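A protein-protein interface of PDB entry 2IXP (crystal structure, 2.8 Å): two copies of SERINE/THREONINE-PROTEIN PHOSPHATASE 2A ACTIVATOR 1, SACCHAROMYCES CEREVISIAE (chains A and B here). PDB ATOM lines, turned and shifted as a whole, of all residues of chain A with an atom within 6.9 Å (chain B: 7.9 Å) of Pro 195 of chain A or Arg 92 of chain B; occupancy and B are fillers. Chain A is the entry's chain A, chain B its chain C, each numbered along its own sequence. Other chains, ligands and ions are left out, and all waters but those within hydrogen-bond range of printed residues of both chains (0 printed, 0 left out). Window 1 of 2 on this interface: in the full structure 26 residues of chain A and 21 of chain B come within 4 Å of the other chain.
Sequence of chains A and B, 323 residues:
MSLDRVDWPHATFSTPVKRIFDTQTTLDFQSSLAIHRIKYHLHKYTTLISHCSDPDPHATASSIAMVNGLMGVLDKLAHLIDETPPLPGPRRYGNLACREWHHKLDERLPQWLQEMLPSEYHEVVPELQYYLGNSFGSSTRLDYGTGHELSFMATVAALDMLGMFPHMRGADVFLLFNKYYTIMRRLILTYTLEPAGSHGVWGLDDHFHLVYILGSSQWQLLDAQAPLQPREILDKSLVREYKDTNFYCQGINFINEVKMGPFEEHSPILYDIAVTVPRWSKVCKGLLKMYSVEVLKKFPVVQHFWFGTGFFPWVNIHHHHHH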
ATOM      1  N   GLY A  94       8.720  -0.705  26.162  1.00  0.00           N
ATOM      2  CA  GLY A  94       7.855  -1.261  27.244  1.00  0.00           C
ATOM      3  C   GLY A  94       6.375  -0.813  27.322  1.00  0.00           C
ATOM      4  O   GLY A  94       6.007   0.223  26.722  1.00  0.00           O
ATOM      5  N   LEU A 142      10.974  -1.739  32.700  1.00  0.00           N
ATOM      6  CA  LEU A 142      10.322  -2.434  31.579  1.00  0.00           C
ATOM      7  C   LEU A 142      11.313  -3.145  30.595  1.00  0.00           C
ATOM      8  O   LEU A 142      11.280  -2.909  29.354  1.00  0.00           O
ATOM      9  CB  LEU A 142       9.413  -1.480  30.791  1.00  0.00           C
ATOM     10  CG  LEU A 142       8.119  -1.041  31.451  1.00  0.00           C
ATOM     11  CD1 LEU A 142       7.566   0.181  30.767  1.00  0.00           C
ATOM     12  CD2 LEU A 142       7.104  -2.141  31.400  1.00  0.00           C
ATOM     13  N   ASP A 143      12.182  -4.006  31.144  1.00  0.00           N
ATOM     14  CA  ASP A 143      13.112  -4.805  30.339  1.00  0.00           C
ATOM     15  C   ASP A 143      13.247  -6.299  30.819  1.00  0.00           C
ATOM     16  O   ASP A 143      12.823  -6.656  31.895  1.00  0.00           O
ATOM     17  CB  ASP A 143      14.455  -4.084  30.268  1.00  0.00           C
ATOM     18  CG  ASP A 143      15.046  -3.827  31.642  1.00  0.00           C
ATOM     19  OD1 ASP A 143      16.016  -3.048  31.776  1.00  0.00           O
ATOM     20  OD2 ASP A 143      14.542  -4.412  32.621  1.00  0.00           O
ATOM     21  N   TYR A 144      13.781  -7.176  29.984  1.00  0.00           N
ATOM     22  CA  TYR A 144      14.204  -8.482  30.444  1.00  0.00           C
ATOM     23  C   TYR A 144      15.594  -8.764  29.929  1.00  0.00           C
ATOM     24  O   TYR A 144      15.893  -8.395  28.799  1.00  0.00           O
ATOM     25  CB  TYR A 144      13.268  -9.591  29.983  1.00  0.00           C
ATOM     26  CG  TYR A 144      13.693 -10.994  30.459  1.00  0.00           C
ATOM     27  CD1 TYR A 144      13.667 -11.352  31.816  1.00  0.00           C
ATOM     28  CD2 TYR A 144      14.090 -11.960  29.558  1.00  0.00           C
ATOM     29  CE1 TYR A 144      14.010 -12.663  32.244  1.00  0.00           C
ATOM     30  CE2 TYR A 144      14.470 -13.251  29.996  1.00  0.00           C
ATOM     31  CZ  TYR A 144      14.412 -13.594  31.323  1.00  0.00           C
ATOM     32  OH  TYR A 144      14.775 -14.854  31.699  1.00  0.00           O
ATOM     33  N   GLY A 145      16.430  -9.417  30.744  1.00  0.00           N
ATOM     34  CA  GLY A 145      17.762  -9.842  30.295  1.00  0.00           C
ATOM     35  C   GLY A 145      18.352 -10.957  31.163  1.00  0.00           C
ATOM     36  O   GLY A 145      17.692 -11.580  32.011  1.00  0.00           O
ATOM     37  N   ILE A 188       7.588 -11.004  27.225  1.00  0.00           N
ATOM     38  CA  ILE A 188       8.260 -10.178  26.280  1.00  0.00           C
ATOM     39  C   ILE A 188       7.289  -9.670  25.188  1.00  0.00           C
ATOM     40  O   ILE A 188       7.135  -8.444  24.972  1.00  0.00           O
ATOM     41  CB  ILE A 188       9.408 -10.879  25.669  1.00  0.00           C
ATOM     42  CG1 ILE A 188      10.458 -11.152  26.763  1.00  0.00           C
ATOM     43  CG2 ILE A 188       9.997  -9.990  24.597  1.00  0.00           C
ATOM     44  CD1 ILE A 188      11.711 -12.006  26.387  1.00  0.00           C
ATOM     45  N   LEU A 189       6.603 -10.578  24.499  1.00  0.00           N
ATOM     46  CA  LEU A 189       5.702 -10.099  23.443  1.00  0.00           C
ATOM     47  C   LEU A 189       4.512  -9.326  23.969  1.00  0.00           C
ATOM     48  O   LEU A 189       4.295  -8.209  23.513  1.00  0.00           O
ATOM     49  CB  LEU A 189       5.287 -11.209  22.469  1.00  0.00           C
ATOM     50  CG  LEU A 189       6.412 -11.598  21.490  1.00  0.00           C
ATOM     51  CD1 LEU A 189       5.941 -12.506  20.297  1.00  0.00           C
ATOM     52  CD2 LEU A 189       7.052 -10.312  20.998  1.00  0.00           C
ATOM     53  N   TYR A 191       3.998  -7.756  26.747  1.00  0.00           N
ATOM     54  CA  TYR A 191       4.410  -6.464  27.372  1.00  0.00           C
ATOM     55  C   TYR A 191       5.405  -5.581  26.591  1.00  0.00           C
ATOM     56  O   TYR A 191       5.483  -4.347  26.815  1.00  0.00           O
ATOM     57  CB  TYR A 191       4.806  -6.633  28.844  1.00  0.00           C
ATOM     58  CG  TYR A 191       3.614  -7.044  29.674  1.00  0.00           C
ATOM     59  CD1 TYR A 191       3.764  -7.929  30.730  1.00  0.00           C
ATOM     60  CD2 TYR A 191       2.342  -6.597  29.364  1.00  0.00           C
ATOM     61  CE1 TYR A 191       2.692  -8.370  31.489  1.00  0.00           C
ATOM     62  CE2 TYR A 191       1.239  -7.021  30.118  1.00  0.00           C
ATOM     63  CZ  TYR A 191       1.413  -7.925  31.203  1.00  0.00           C
ATOM     64  OH  TYR A 191       0.336  -8.364  32.009  1.00  0.00           O
ATOM     65  N   THR A 192       6.169  -6.191  25.676  1.00  0.00           N
ATOM     66  CA  THR A 192       6.923  -5.385  24.758  1.00  0.00           C
ATOM     67  C   THR A 192       8.089  -4.975  25.636  1.00  0.00           C
ATOM     68  O   THR A 192       8.416  -3.807  25.774  1.00  0.00           O
ATOM     69  CB  THR A 192       5.937  -4.239  24.216  1.00  0.00           C
ATOM     70  OG1 THR A 192       5.101  -4.762  23.151  1.00  0.00           O
ATOM     71  CG2 THR A 192       6.646  -2.910  23.823  1.00  0.00           C
ATOM     72  N   LEU A 193       8.686  -5.972  26.279  1.00  0.00           N
ATOM     73  CA  LEU A 193       9.771  -5.733  27.220  1.00  0.00           C
ATOM     74  C   LEU A 193      11.090  -5.628  26.442  1.00  0.00           C
ATOM     75  O   LEU A 193      11.345  -6.403  25.499  1.00  0.00           O
ATOM     76  CB  LEU A 193       9.815  -6.829  28.283  1.00  0.00           C
ATOM     77  CG  LEU A 193       8.578  -7.190  29.133  1.00  0.00           C
ATOM     78  CD1 LEU A 193       8.989  -7.901  30.441  1.00  0.00           C
ATOM     79  CD2 LEU A 193       7.641  -5.949  29.479  1.00  0.00           C
ATOM     80  N   GLU A 194      11.895  -4.627  26.804  1.00  0.00           N
ATOM     81  CA  GLU A 194      13.132  -4.315  26.093  1.00  0.00           C
ATOM     82  C   GLU A 194      14.244  -5.194  26.593  1.00  0.00           C
ATOM     83  O   GLU A 194      14.076  -5.894  27.572  1.00  0.00           O
ATOM     84  CB  GLU A 194      13.542  -2.854  26.301  1.00  0.00           C
ATOM     85  CG  GLU A 194      12.613  -1.771  25.695  1.00  0.00           C
ATOM     86  CD  GLU A 194      12.440  -1.907  24.169  1.00  0.00           C
ATOM     87  OE1 GLU A 194      13.195  -2.674  23.564  1.00  0.00           O
ATOM     88  OE2 GLU A 194      11.538  -1.266  23.572  1.00  0.00           O
ATOM     89  N   PRO A 195      15.399  -5.170  25.903  1.00  0.00           N
ATOM     90  CA  PRO A 195      16.491  -5.986  26.327  1.00  0.00           C
ATOM     91  C   PRO A 195      17.248  -5.398  27.538  1.00  0.00           C
ATOM     92  O   PRO A 195      17.834  -4.312  27.463  1.00  0.00           O
ATOM     93  CB  PRO A 195      17.344  -6.011  25.075  1.00  0.00           C
ATOM     94  CG  PRO A 195      16.477  -5.513  24.019  1.00  0.00           C
ATOM     95  CD  PRO A 195      15.771  -4.485  24.662  1.00  0.00           C
ATOM     96  N   ALA A 196      17.245  -6.128  28.654  1.00  0.00           N
ATOM     97  CA  ALA A 196      17.893  -5.640  29.910  1.00  0.00           C
ATOM     98  C   ALA A 196      19.341  -6.021  30.058  1.00  0.00           C
ATOM     99  O   ALA A 196      19.608  -7.181  30.305  1.00  0.00           O
ATOM    100  CB  ALA A 196      17.148  -6.120  31.133  1.00  0.00           C
ATOM    101  N   GLY A 197      20.234  -5.047  29.918  1.00  0.00           N
ATOM    102  CA  GLY A 197      21.638  -5.174  30.195  1.00  0.00           C
ATOM    103  C   GLY A 197      22.351  -5.818  29.029  1.00  0.00           C
ATOM    104  O   GLY A 197      23.221  -6.662  29.281  1.00  0.00           O
ATOM    105  N   SER A 198      22.037  -5.460  27.764  1.00  0.00           N
ATOM    106  CA  SER A 198      22.491  -6.334  26.648  1.00  0.00           C
ATOM    107  C   SER A 198      23.674  -5.776  25.947  1.00  0.00           C
ATOM    108  O   SER A 198      23.936  -4.597  26.177  1.00  0.00           O
ATOM    109  CB  SER A 198      21.364  -6.617  25.663  1.00  0.00           C
ATOM    110  OG  SER A 198      21.381  -5.740  24.565  1.00  0.00           O
ATOM    111  N   ASP A 205      22.435 -13.355  23.000  1.00  0.00           N
ATOM    112  CA  ASP A 205      21.019 -13.275  22.653  1.00  0.00           C
ATOM    113  C   ASP A 205      20.549 -12.010  23.333  1.00  0.00           C
ATOM    114  O   ASP A 205      21.105 -11.649  24.337  1.00  0.00           O
ATOM    115  CB  ASP A 205      20.287 -14.530  23.170  1.00  0.00           C
ATOM    116  CG  ASP A 205      18.787 -14.540  22.894  1.00  0.00           C
ATOM    117  OD1 ASP A 205      18.323 -15.450  22.145  1.00  0.00           O
ATOM    118  OD2 ASP A 205      18.061 -13.673  23.457  1.00  0.00           O
ATOM    119  N   ASP A 206      19.536 -11.343  22.778  1.00  0.00           N
ATOM    120  CA  ASP A 206      19.040 -10.047  23.280  1.00  0.00           C
ATOM    121  C   ASP A 206      18.761 -10.173  24.738  1.00  0.00           C
ATOM    122  O   ASP A 206      18.978  -9.222  25.446  1.00  0.00           O
ATOM    123  CB  ASP A 206      17.672  -9.677  22.666  1.00  0.00           C
ATOM    124  CG  ASP A 206      17.745  -8.823  21.377  1.00  0.00           C
ATOM    125  OD1 ASP A 206      18.745  -8.874  20.619  1.00  0.00           O
ATOM    126  OD2 ASP A 206      16.739  -8.107  21.120  1.00  0.00           O
ATOM    127  N   HIS A 207      18.336 -11.377  25.171  1.00  0.00           N
ATOM    128  CA  HIS A 207      17.545 -11.629  26.417  1.00  0.00           C
ATOM    129  C   HIS A 207      17.917 -12.810  27.331  1.00  0.00           C
ATOM    130  O   HIS A 207      17.618 -12.750  28.529  1.00  0.00           O
ATOM    131  CB  HIS A 207      16.119 -11.931  26.006  1.00  0.00           C
ATOM    132  CG  HIS A 207      15.345 -10.745  25.532  1.00  0.00           C
ATOM    133  ND1 HIS A 207      14.733 -10.704  24.292  1.00  0.00           N
ATOM    134  CD2 HIS A 207      15.020  -9.584  26.147  1.00  0.00           C
ATOM    135  CE1 HIS A 207      14.085  -9.559  24.149  1.00  0.00           C
ATOM    136  NE2 HIS A 207      14.251  -8.859  25.258  1.00  0.00           N
ATOM    137  N   VAL A 258      10.848 -13.359  15.701  1.00  0.00           N
ATOM    138  CA  VAL A 258      10.866 -12.012  16.220  1.00  0.00           C
ATOM    139  C   VAL A 258      11.774 -11.025  15.423  1.00  0.00           C
ATOM    140  O   VAL A 258      11.306  -9.938  15.061  1.00  0.00           O
ATOM    141  CB  VAL A 258      11.334 -12.129  17.676  1.00  0.00           C
ATOM    142  CG1 VAL A 258      12.546 -11.171  18.003  1.00  0.00           C
ATOM    143  CG2 VAL A 258      10.136 -12.052  18.626  1.00  0.00           C
ATOM    144  N   LYS A 259      13.052 -11.396  15.179  1.00  0.00           N
ATOM    145  CA  LYS A 259      13.990 -10.615  14.358  1.00  0.00           C
ATOM    146  C   LYS A 259      13.860 -10.856  12.868  1.00  0.00           C
ATOM    147  O   LYS A 259      13.924 -11.960  12.443  1.00  0.00           O
ATOM    148  CB  LYS A 259      15.424 -10.898  14.733  1.00  0.00           C
ATOM    149  CG  LYS A 259      15.908 -10.163  15.930  1.00  0.00           C
ATOM    150  CD  LYS A 259      17.198 -10.764  16.358  1.00  0.00           C
ATOM    151  CE  LYS A 259      17.549 -10.376  17.729  1.00  0.00           C
ATOM    152  NZ  LYS A 259      17.960  -8.974  17.677  1.00  0.00           N
ATOM    153  N   GLY B  89      -0.718  -4.219  16.226  1.00  0.00           N
ATOM    154  CA  GLY B  89       0.040  -5.283  16.956  1.00  0.00           C
ATOM    155  C   GLY B  89       1.151  -4.851  17.927  1.00  0.00           C
ATOM    156  O   GLY B  89       1.219  -3.669  18.319  1.00  0.00           O
ATOM    157  N   PRO B  90       2.058  -5.789  18.308  1.00  0.00           N
ATOM    158  CA  PRO B  90       2.962  -5.478  19.427  1.00  0.00           C
ATOM    159  C   PRO B  90       4.131  -4.562  19.064  1.00  0.00           C
ATOM    160  O   PRO B  90       5.059  -5.004  18.369  1.00  0.00           O
ATOM    161  CB  PRO B  90       3.457  -6.861  19.906  1.00  0.00           C
ATOM    162  CG  PRO B  90       3.221  -7.796  18.785  1.00  0.00           C
ATOM    163  CD  PRO B  90       2.332  -7.124  17.737  1.00  0.00           C
ATOM    164  N   ARG B  91       4.036  -3.305  19.553  1.00  0.00           N
ATOM    165  CA  ARG B  91       5.087  -2.224  19.575  1.00  0.00           C
ATOM    166  C   ARG B  91       6.528  -2.768  19.884  1.00  0.00           C
ATOM    167  O   ARG B  91       7.386  -2.015  20.308  1.00  0.00           O
ATOM    168  CB  ARG B  91       4.667  -1.073  20.592  1.00  0.00           C
ATOM    169  CG  ARG B  91       4.840   0.496  20.187  1.00  0.00           C
ATOM    170  CD  ARG B  91       5.223   1.545  21.366  1.00  0.00           C
ATOM    171  NE  ARG B  91       4.064   2.095  22.063  1.00  0.00           N
ATOM    172  CZ  ARG B  91       3.341   1.445  22.998  1.00  0.00           C
ATOM    173  NH1 ARG B  91       3.671   0.209  23.391  1.00  0.00           N
ATOM    174  NH2 ARG B  91       2.265   2.016  23.562  1.00  0.00           N
ATOM    175  N   ARG B  92       6.817  -4.052  19.665  1.00  0.00           N
ATOM    176  CA  ARG B  92       8.105  -4.596  20.120  1.00  0.00           C
ATOM    177  C   ARG B  92       9.275  -4.692  19.088  1.00  0.00           C
ATOM    178  O   ARG B  92      10.413  -4.330  19.430  1.00  0.00           O
ATOM    179  CB  ARG B  92       7.912  -5.923  20.878  1.00  0.00           C
ATOM    180  CG  ARG B  92       8.905  -6.113  22.057  1.00  0.00           C
ATOM    181  CD  ARG B  92      10.372  -6.133  21.569  1.00  0.00           C
ATOM    182  NE  ARG B  92      11.370  -6.357  22.600  1.00  0.00           N
ATOM    183  CZ  ARG B  92      12.682  -6.288  22.393  1.00  0.00           C
ATOM    184  NH1 ARG B  92      13.200  -5.997  21.196  1.00  0.00           N
ATOM    185  NH2 ARG B  92      13.499  -6.522  23.397  1.00  0.00           N
ATOM    186  N   TYR B  93       9.019  -5.179  17.863  1.00  0.00           N
ATOM    187  CA  TYR B  93      10.066  -5.235  16.792  1.00  0.00           C
ATOM    188  C   TYR B  93       9.850  -4.280  15.593  1.00  0.00           C
ATOM    189  O   TYR B  93       8.903  -3.495  15.603  1.00  0.00           O
ATOM    190  CB  TYR B  93      10.260  -6.675  16.335  1.00  0.00           C
ATOM    191  CG  TYR B  93      10.673  -7.493  17.499  1.00  0.00           C
ATOM    192  CD1 TYR B  93       9.741  -8.271  18.174  1.00  0.00           C
ATOM    193  CD2 TYR B  93      11.998  -7.443  17.965  1.00  0.00           C
ATOM    194  CE1 TYR B  93      10.107  -8.982  19.265  1.00  0.00           C
ATOM    195  CE2 TYR B  93      12.386  -8.157  19.049  1.00  0.00           C
ATOM    196  CZ  TYR B  93      11.432  -8.927  19.709  1.00  0.00           C
ATOM    197  OH  TYR B  93      11.786  -9.655  20.819  1.00  0.00           O
ATOM    198  N   GLY B  94      10.726  -4.324  14.583  1.00  0.00           N
ATOM    199  CA  GLY B  94      10.444  -3.676  13.296  1.00  0.00           C
ATOM    200  C   GLY B  94       8.971  -3.871  12.893  1.00  0.00           C
ATOM    201  O   GLY B  94       8.453  -5.010  12.811  1.00  0.00           O
ATOM    202  N   ASN B  95       8.267  -2.764  12.690  1.00  0.00           N
ATOM    203  CA  ASN B  95       6.893  -2.879  12.290  1.00  0.00           C
ATOM    204  C   ASN B  95       6.868  -3.031  10.800  1.00  0.00           C
ATOM    205  O   ASN B  95       7.508  -2.283  10.092  1.00  0.00           O
ATOM    206  CB  ASN B  95       6.065  -1.685  12.738  1.00  0.00           C
ATOM    207  CG  ASN B  95       4.765  -1.609  12.030  1.00  0.00           C
ATOM    208  OD1 ASN B  95       4.734  -1.557  10.806  1.00  0.00           O
ATOM    209  ND2 ASN B  95       3.675  -1.608  12.779  1.00  0.00           N
ATOM    210  N   TYR B 191       7.516   3.132  12.769  1.00  0.00           N
ATOM    211  CA  TYR B 191       7.862   1.796  12.289  1.00  0.00           C
ATOM    212  C   TYR B 191       8.568   0.997  13.369  1.00  0.00           C
ATOM    213  O   TYR B 191       8.855  -0.189  13.214  1.00  0.00           O
ATOM    214  CB  TYR B 191       8.656   1.907  10.989  1.00  0.00           C
ATOM    215  CG  TYR B 191       7.816   2.550   9.904  1.00  0.00           C
ATOM    216  CD1 TYR B 191       8.363   3.454   9.015  1.00  0.00           C
ATOM    217  CD2 TYR B 191       6.451   2.273   9.803  1.00  0.00           C
ATOM    218  CE1 TYR B 191       7.594   4.051   8.043  1.00  0.00           C
ATOM    219  CE2 TYR B 191       5.673   2.878   8.830  1.00  0.00           C
ATOM    220  CZ  TYR B 191       6.248   3.773   7.949  1.00  0.00           C
ATOM    221  OH  TYR B 191       5.474   4.371   6.962  1.00  0.00           O
ATOM    222  N   THR B 192       8.790   1.668  14.493  1.00  0.00           N
ATOM    223  CA  THR B 192       8.992   0.988  15.742  1.00  0.00           C
ATOM    224  C   THR B 192      10.280   0.146  15.594  1.00  0.00           C
ATOM    225  O   THR B 192      10.345  -1.002  15.996  1.00  0.00           O
ATOM    226  CB  THR B 192       7.640   0.295  16.104  1.00  0.00           C
ATOM    227  OG1 THR B 192       7.472   0.203  17.510  1.00  0.00           O
ATOM    228  CG2 THR B 192       7.376  -1.051  15.417  1.00  0.00           C
ATOM    229  N   LEU B 193      11.312   0.792  15.029  1.00  0.00           N
ATOM    230  CA  LEU B 193      12.456   0.135  14.429  1.00  0.00           C
ATOM    231  C   LEU B 193      13.458  -0.314  15.433  1.00  0.00           C
ATOM    232  O   LEU B 193      13.615   0.303  16.458  1.00  0.00           O
ATOM    233  CB  LEU B 193      13.160   1.046  13.447  1.00  0.00           C
ATOM    234  CG  LEU B 193      12.490   1.621  12.190  1.00  0.00           C
ATOM    235  CD1 LEU B 193      13.493   2.416  11.284  1.00  0.00           C
ATOM    236  CD2 LEU B 193      11.787   0.563  11.394  1.00  0.00           C
ATOM    237  N   GLU B 194      14.129  -1.411  15.116  1.00  0.00           N
ATOM    238  CA  GLU B 194      15.085  -2.047  15.992  1.00  0.00           C
ATOM    239  C   GLU B 194      16.393  -1.296  15.715  1.00  0.00           C
ATOM    240  O   GLU B 194      16.568  -0.716  14.643  1.00  0.00           O
ATOM    241  CB  GLU B 194      15.245  -3.556  15.656  1.00  0.00           C
ATOM    242  CG  GLU B 194      13.980  -4.497  15.714  1.00  0.00           C
ATOM    243  CD  GLU B 194      14.179  -5.992  15.041  1.00  0.00           C
ATOM    244  OE1 GLU B 194      15.356  -6.525  15.017  1.00  0.00           O
ATOM    245  OE2 GLU B 194      13.173  -6.636  14.547  1.00  0.00           O
ATOM    246  N   PRO B 195      17.317  -1.264  16.684  1.00  0.00           N
ATOM    247  CA  PRO B 195      18.677  -0.739  16.421  1.00  0.00           C
ATOM    248  C   PRO B 195      19.601  -1.647  15.596  1.00  0.00           C
ATOM    249  O   PRO B 195      19.595  -2.863  15.846  1.00  0.00           O
ATOM    250  CB  PRO B 195      19.240  -0.588  17.831  1.00  0.00           C
ATOM    251  CG  PRO B 195      18.455  -1.505  18.667  1.00  0.00           C
ATOM    252  CD  PRO B 195      17.099  -1.595  18.098  1.00  0.00           C
ATOM    253  N   SER B 198      23.936  -2.031  16.996  1.00  0.00           N
ATOM    254  CA  SER B 198      23.837  -1.637  18.381  1.00  0.00           C
ATOM    255  C   SER B 198      24.857  -2.408  19.256  1.00  0.00           C
ATOM    256  O   SER B 198      25.139  -3.617  19.065  1.00  0.00           O
ATOM    257  CB  SER B 198      22.387  -1.802  18.821  1.00  0.00           C
ATOM    258  OG  SER B 198      22.220  -1.856  20.224  1.00  0.00           O
ATOM    259  N   GLY B 200      24.482  -2.378  22.401  1.00  0.00           N
ATOM    260  CA  GLY B 200      23.692  -2.457  23.614  1.00  0.00           C
ATOM    261  C   GLY B 200      24.001  -1.284  24.524  1.00  0.00           C
ATOM    262  O   GLY B 200      24.409  -0.229  24.104  1.00  0.00           O
ATOM    263  N   VAL B 201      23.801  -1.522  25.792  1.00  0.00           N
ATOM    264  CA  VAL B 201      24.240  -0.735  26.915  1.00  0.00           C
ATOM    265  C   VAL B 201      25.794  -0.479  26.954  1.00  0.00           C
ATOM    266  O   VAL B 201      26.350  -0.015  27.942  1.00  0.00           O
ATOM    267  CB  VAL B 201      23.754  -1.561  28.144  1.00  0.00           C
ATOM    268  CG1 VAL B 201      24.873  -2.419  28.768  1.00  0.00           C
ATOM    269  CG2 VAL B 201      23.056  -0.713  29.128  1.00  0.00           C
ATOM    270  N   ASP B 206      21.403   3.952  20.787  1.00  0.00           N
ATOM    271  CA  ASP B 206      20.931   2.786  20.020  1.00  0.00           C
ATOM    272  C   ASP B 206      21.005   3.030  18.519  1.00  0.00           C
ATOM    273  O   ASP B 206      21.342   2.117  17.767  1.00  0.00           O
ATOM    274  CB  ASP B 206      19.482   2.407  20.419  1.00  0.00           C
ATOM    275  CG  ASP B 206      19.400   1.622  21.764  1.00  0.00           C
ATOM    276  OD1 ASP B 206      20.400   0.955  22.149  1.00  0.00           O
ATOM    277  OD2 ASP B 206      18.328   1.648  22.412  1.00  0.00           O
ATOM    278  N   LYS B 259      12.950   5.397  26.379  1.00  0.00           N
ATOM    279  CA  LYS B 259      13.541   4.383  27.234  1.00  0.00           C
ATOM    280  C   LYS B 259      13.163   4.665  28.675  1.00  0.00           C
ATOM    281  O   LYS B 259      13.162   5.806  29.109  1.00  0.00           O
ATOM    282  CB  LYS B 259      15.058   4.398  27.045  1.00  0.00           C
ATOM    283  CG  LYS B 259      15.661   3.430  25.990  1.00  0.00           C
ATOM    284  CD  LYS B 259      17.111   3.850  25.760  1.00  0.00           C
ATOM    285  CE  LYS B 259      17.951   2.838  24.992  1.00  0.00           C
ATOM    286  NZ  LYS B 259      18.467   1.738  25.829  1.00  0.00           N
ATOM    287  N   HIS B 266      20.363   2.901  31.817  1.00  0.00           N
ATOM    288  CA  HIS B 266      20.111   2.515  30.451  1.00  0.00           C
ATOM    289  C   HIS B 266      21.051   3.159  29.470  1.00  0.00           C
ATOM    290  O   HIS B 266      21.207   2.663  28.353  1.00  0.00           O
ATOM    291  CB  HIS B 266      18.641   2.693  30.014  1.00  0.00           C
ATOM    292  CG  HIS B 266      18.167   4.119  29.913  1.00  0.00           C
ATOM    293  ND1 HIS B 266      17.178   4.641  30.741  1.00  0.00           N
ATOM    294  CD2 HIS B 266      18.503   5.111  29.053  1.00  0.00           C
ATOM    295  CE1 HIS B 266      16.959   5.903  30.414  1.00  0.00           C
ATOM    296  NE2 HIS B 266      17.755   6.213  29.398  1.00  0.00           N
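OE1 of Glu 194 of chain A is in salt-bridge range of NH2 of Arg 92 of chain B (3.9 Å).
The backbone carbonyl oxygen (O) of Leu 193 of chain A is in hydrogen-bond range of the guanidinium group (NE) of Arg 92 of chain B (2.9 Å).
N of Pro 195 of chain A lies close to NH2 of Arg 92 of chain B (3.4 Å).
The backbone carbonyl oxygen (O) of Ser 198 of chain A sits at hydrogen-bond distance from the backbone NH (N) of Val 201 of chain B (3.1 Å).
NE2 of His 207 of chain A is in hydrogen-bond range of NH2 of Arg 92 of chain B (3.1 Å).
The side-chain amino group of Lys 259 of chain A is in salt-bridge range of the side-chain carboxylate of Asp 206 of chain A (3.0 Å).
The backbone carbonyl oxygen (O) of Glu 194 of chain A is in hydrogen-bond range of the backbone NH (N) of Tyr 144 of chain A.
The backbone carbonyl oxygen (O) of Ile 188 of chain A is in hydrogen-bond range of the backbone NH (N) of Leu 193 of chain A, 3.2 Å away.
The side-chain hydroxyl of Ser 198 of chain B lies close to the backbone NH of Gly 200 of chain B.
N of Gly 94 of chain B is in hydrogen-bond range of OE2 of Glu 194 of chain B (3.4 Å).
The backbone carbonyl oxygen (O) of Leu 142 of chain A is in hydrogen-bond range of the backbone NH (N) of Glu 194 of chain A, 3.1 Å away.
Among the printed residues, merely in contact across the chains: Val 258 of chain A with Tyr 93 of chain B (3.0 Å), Ser 198 of chain A with Gly 200 of chain B (3.3 Å), Thr 192 of chain A with Arg 92 of chain B (3.4 Å), Thr 192 of chain A with Arg 91 of chain B (3.7 Å), Leu 189 of chain A with Tyr 93 of chain B (3.8 Å), Lys 259 of chain A with Glu 194 of chain B (3.8 Å), Val 258 of chain A with Glu 194 of chain B (3.8 Å) and Leu 189 of chain A with Pro 90 of chain B (3.9 Å).
Of the printed residues of chain B, Leu 189 of chain A touches Pro 90 (3.9 Å) and Tyr 93 (3.8 Å).
Printed residues of chain B within 4 Å of Thr 192 of chain A: Arg 91 and Arg 92.
Of the printed residues of chain B, Leu 193 of chain A touches Arg 92 (2.9 Å).
Of the printed residues of chain B, Pro 195 of chain A touches Arg 92 (3.2 Å).
Asp 206 of chain A touches none of the printed residues of chain B.
Arg 92 of chain B touches just these residues of chain A: Thr 192, Leu 193, Glu 194, Pro 195 and His 207.
Pro 195 of chain B touches none of the printed residues of chain A.
The nearest residue of chain B that does not touch Pro 195 of chain A is Lys 259 of chain B (6.3 Å).
The nearest printed residue of chain A that does not touch Arg 92 of chain B is Asp 206 of chain A (4.1 Å).
The nearest printed residue of chain B that does not touch Lys 259 of chain A is Tyr 93 of chain B (4.9 Å).
Among the printed residues, 13 pairs touch across the chains.
Lys 259 of chain A touches Glu 194 of chain B, but with the chains exchanged Glu 194 of chain A does not touch Lys 259 of chain B (6.0 Å).
9 positions are printed for both chains.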
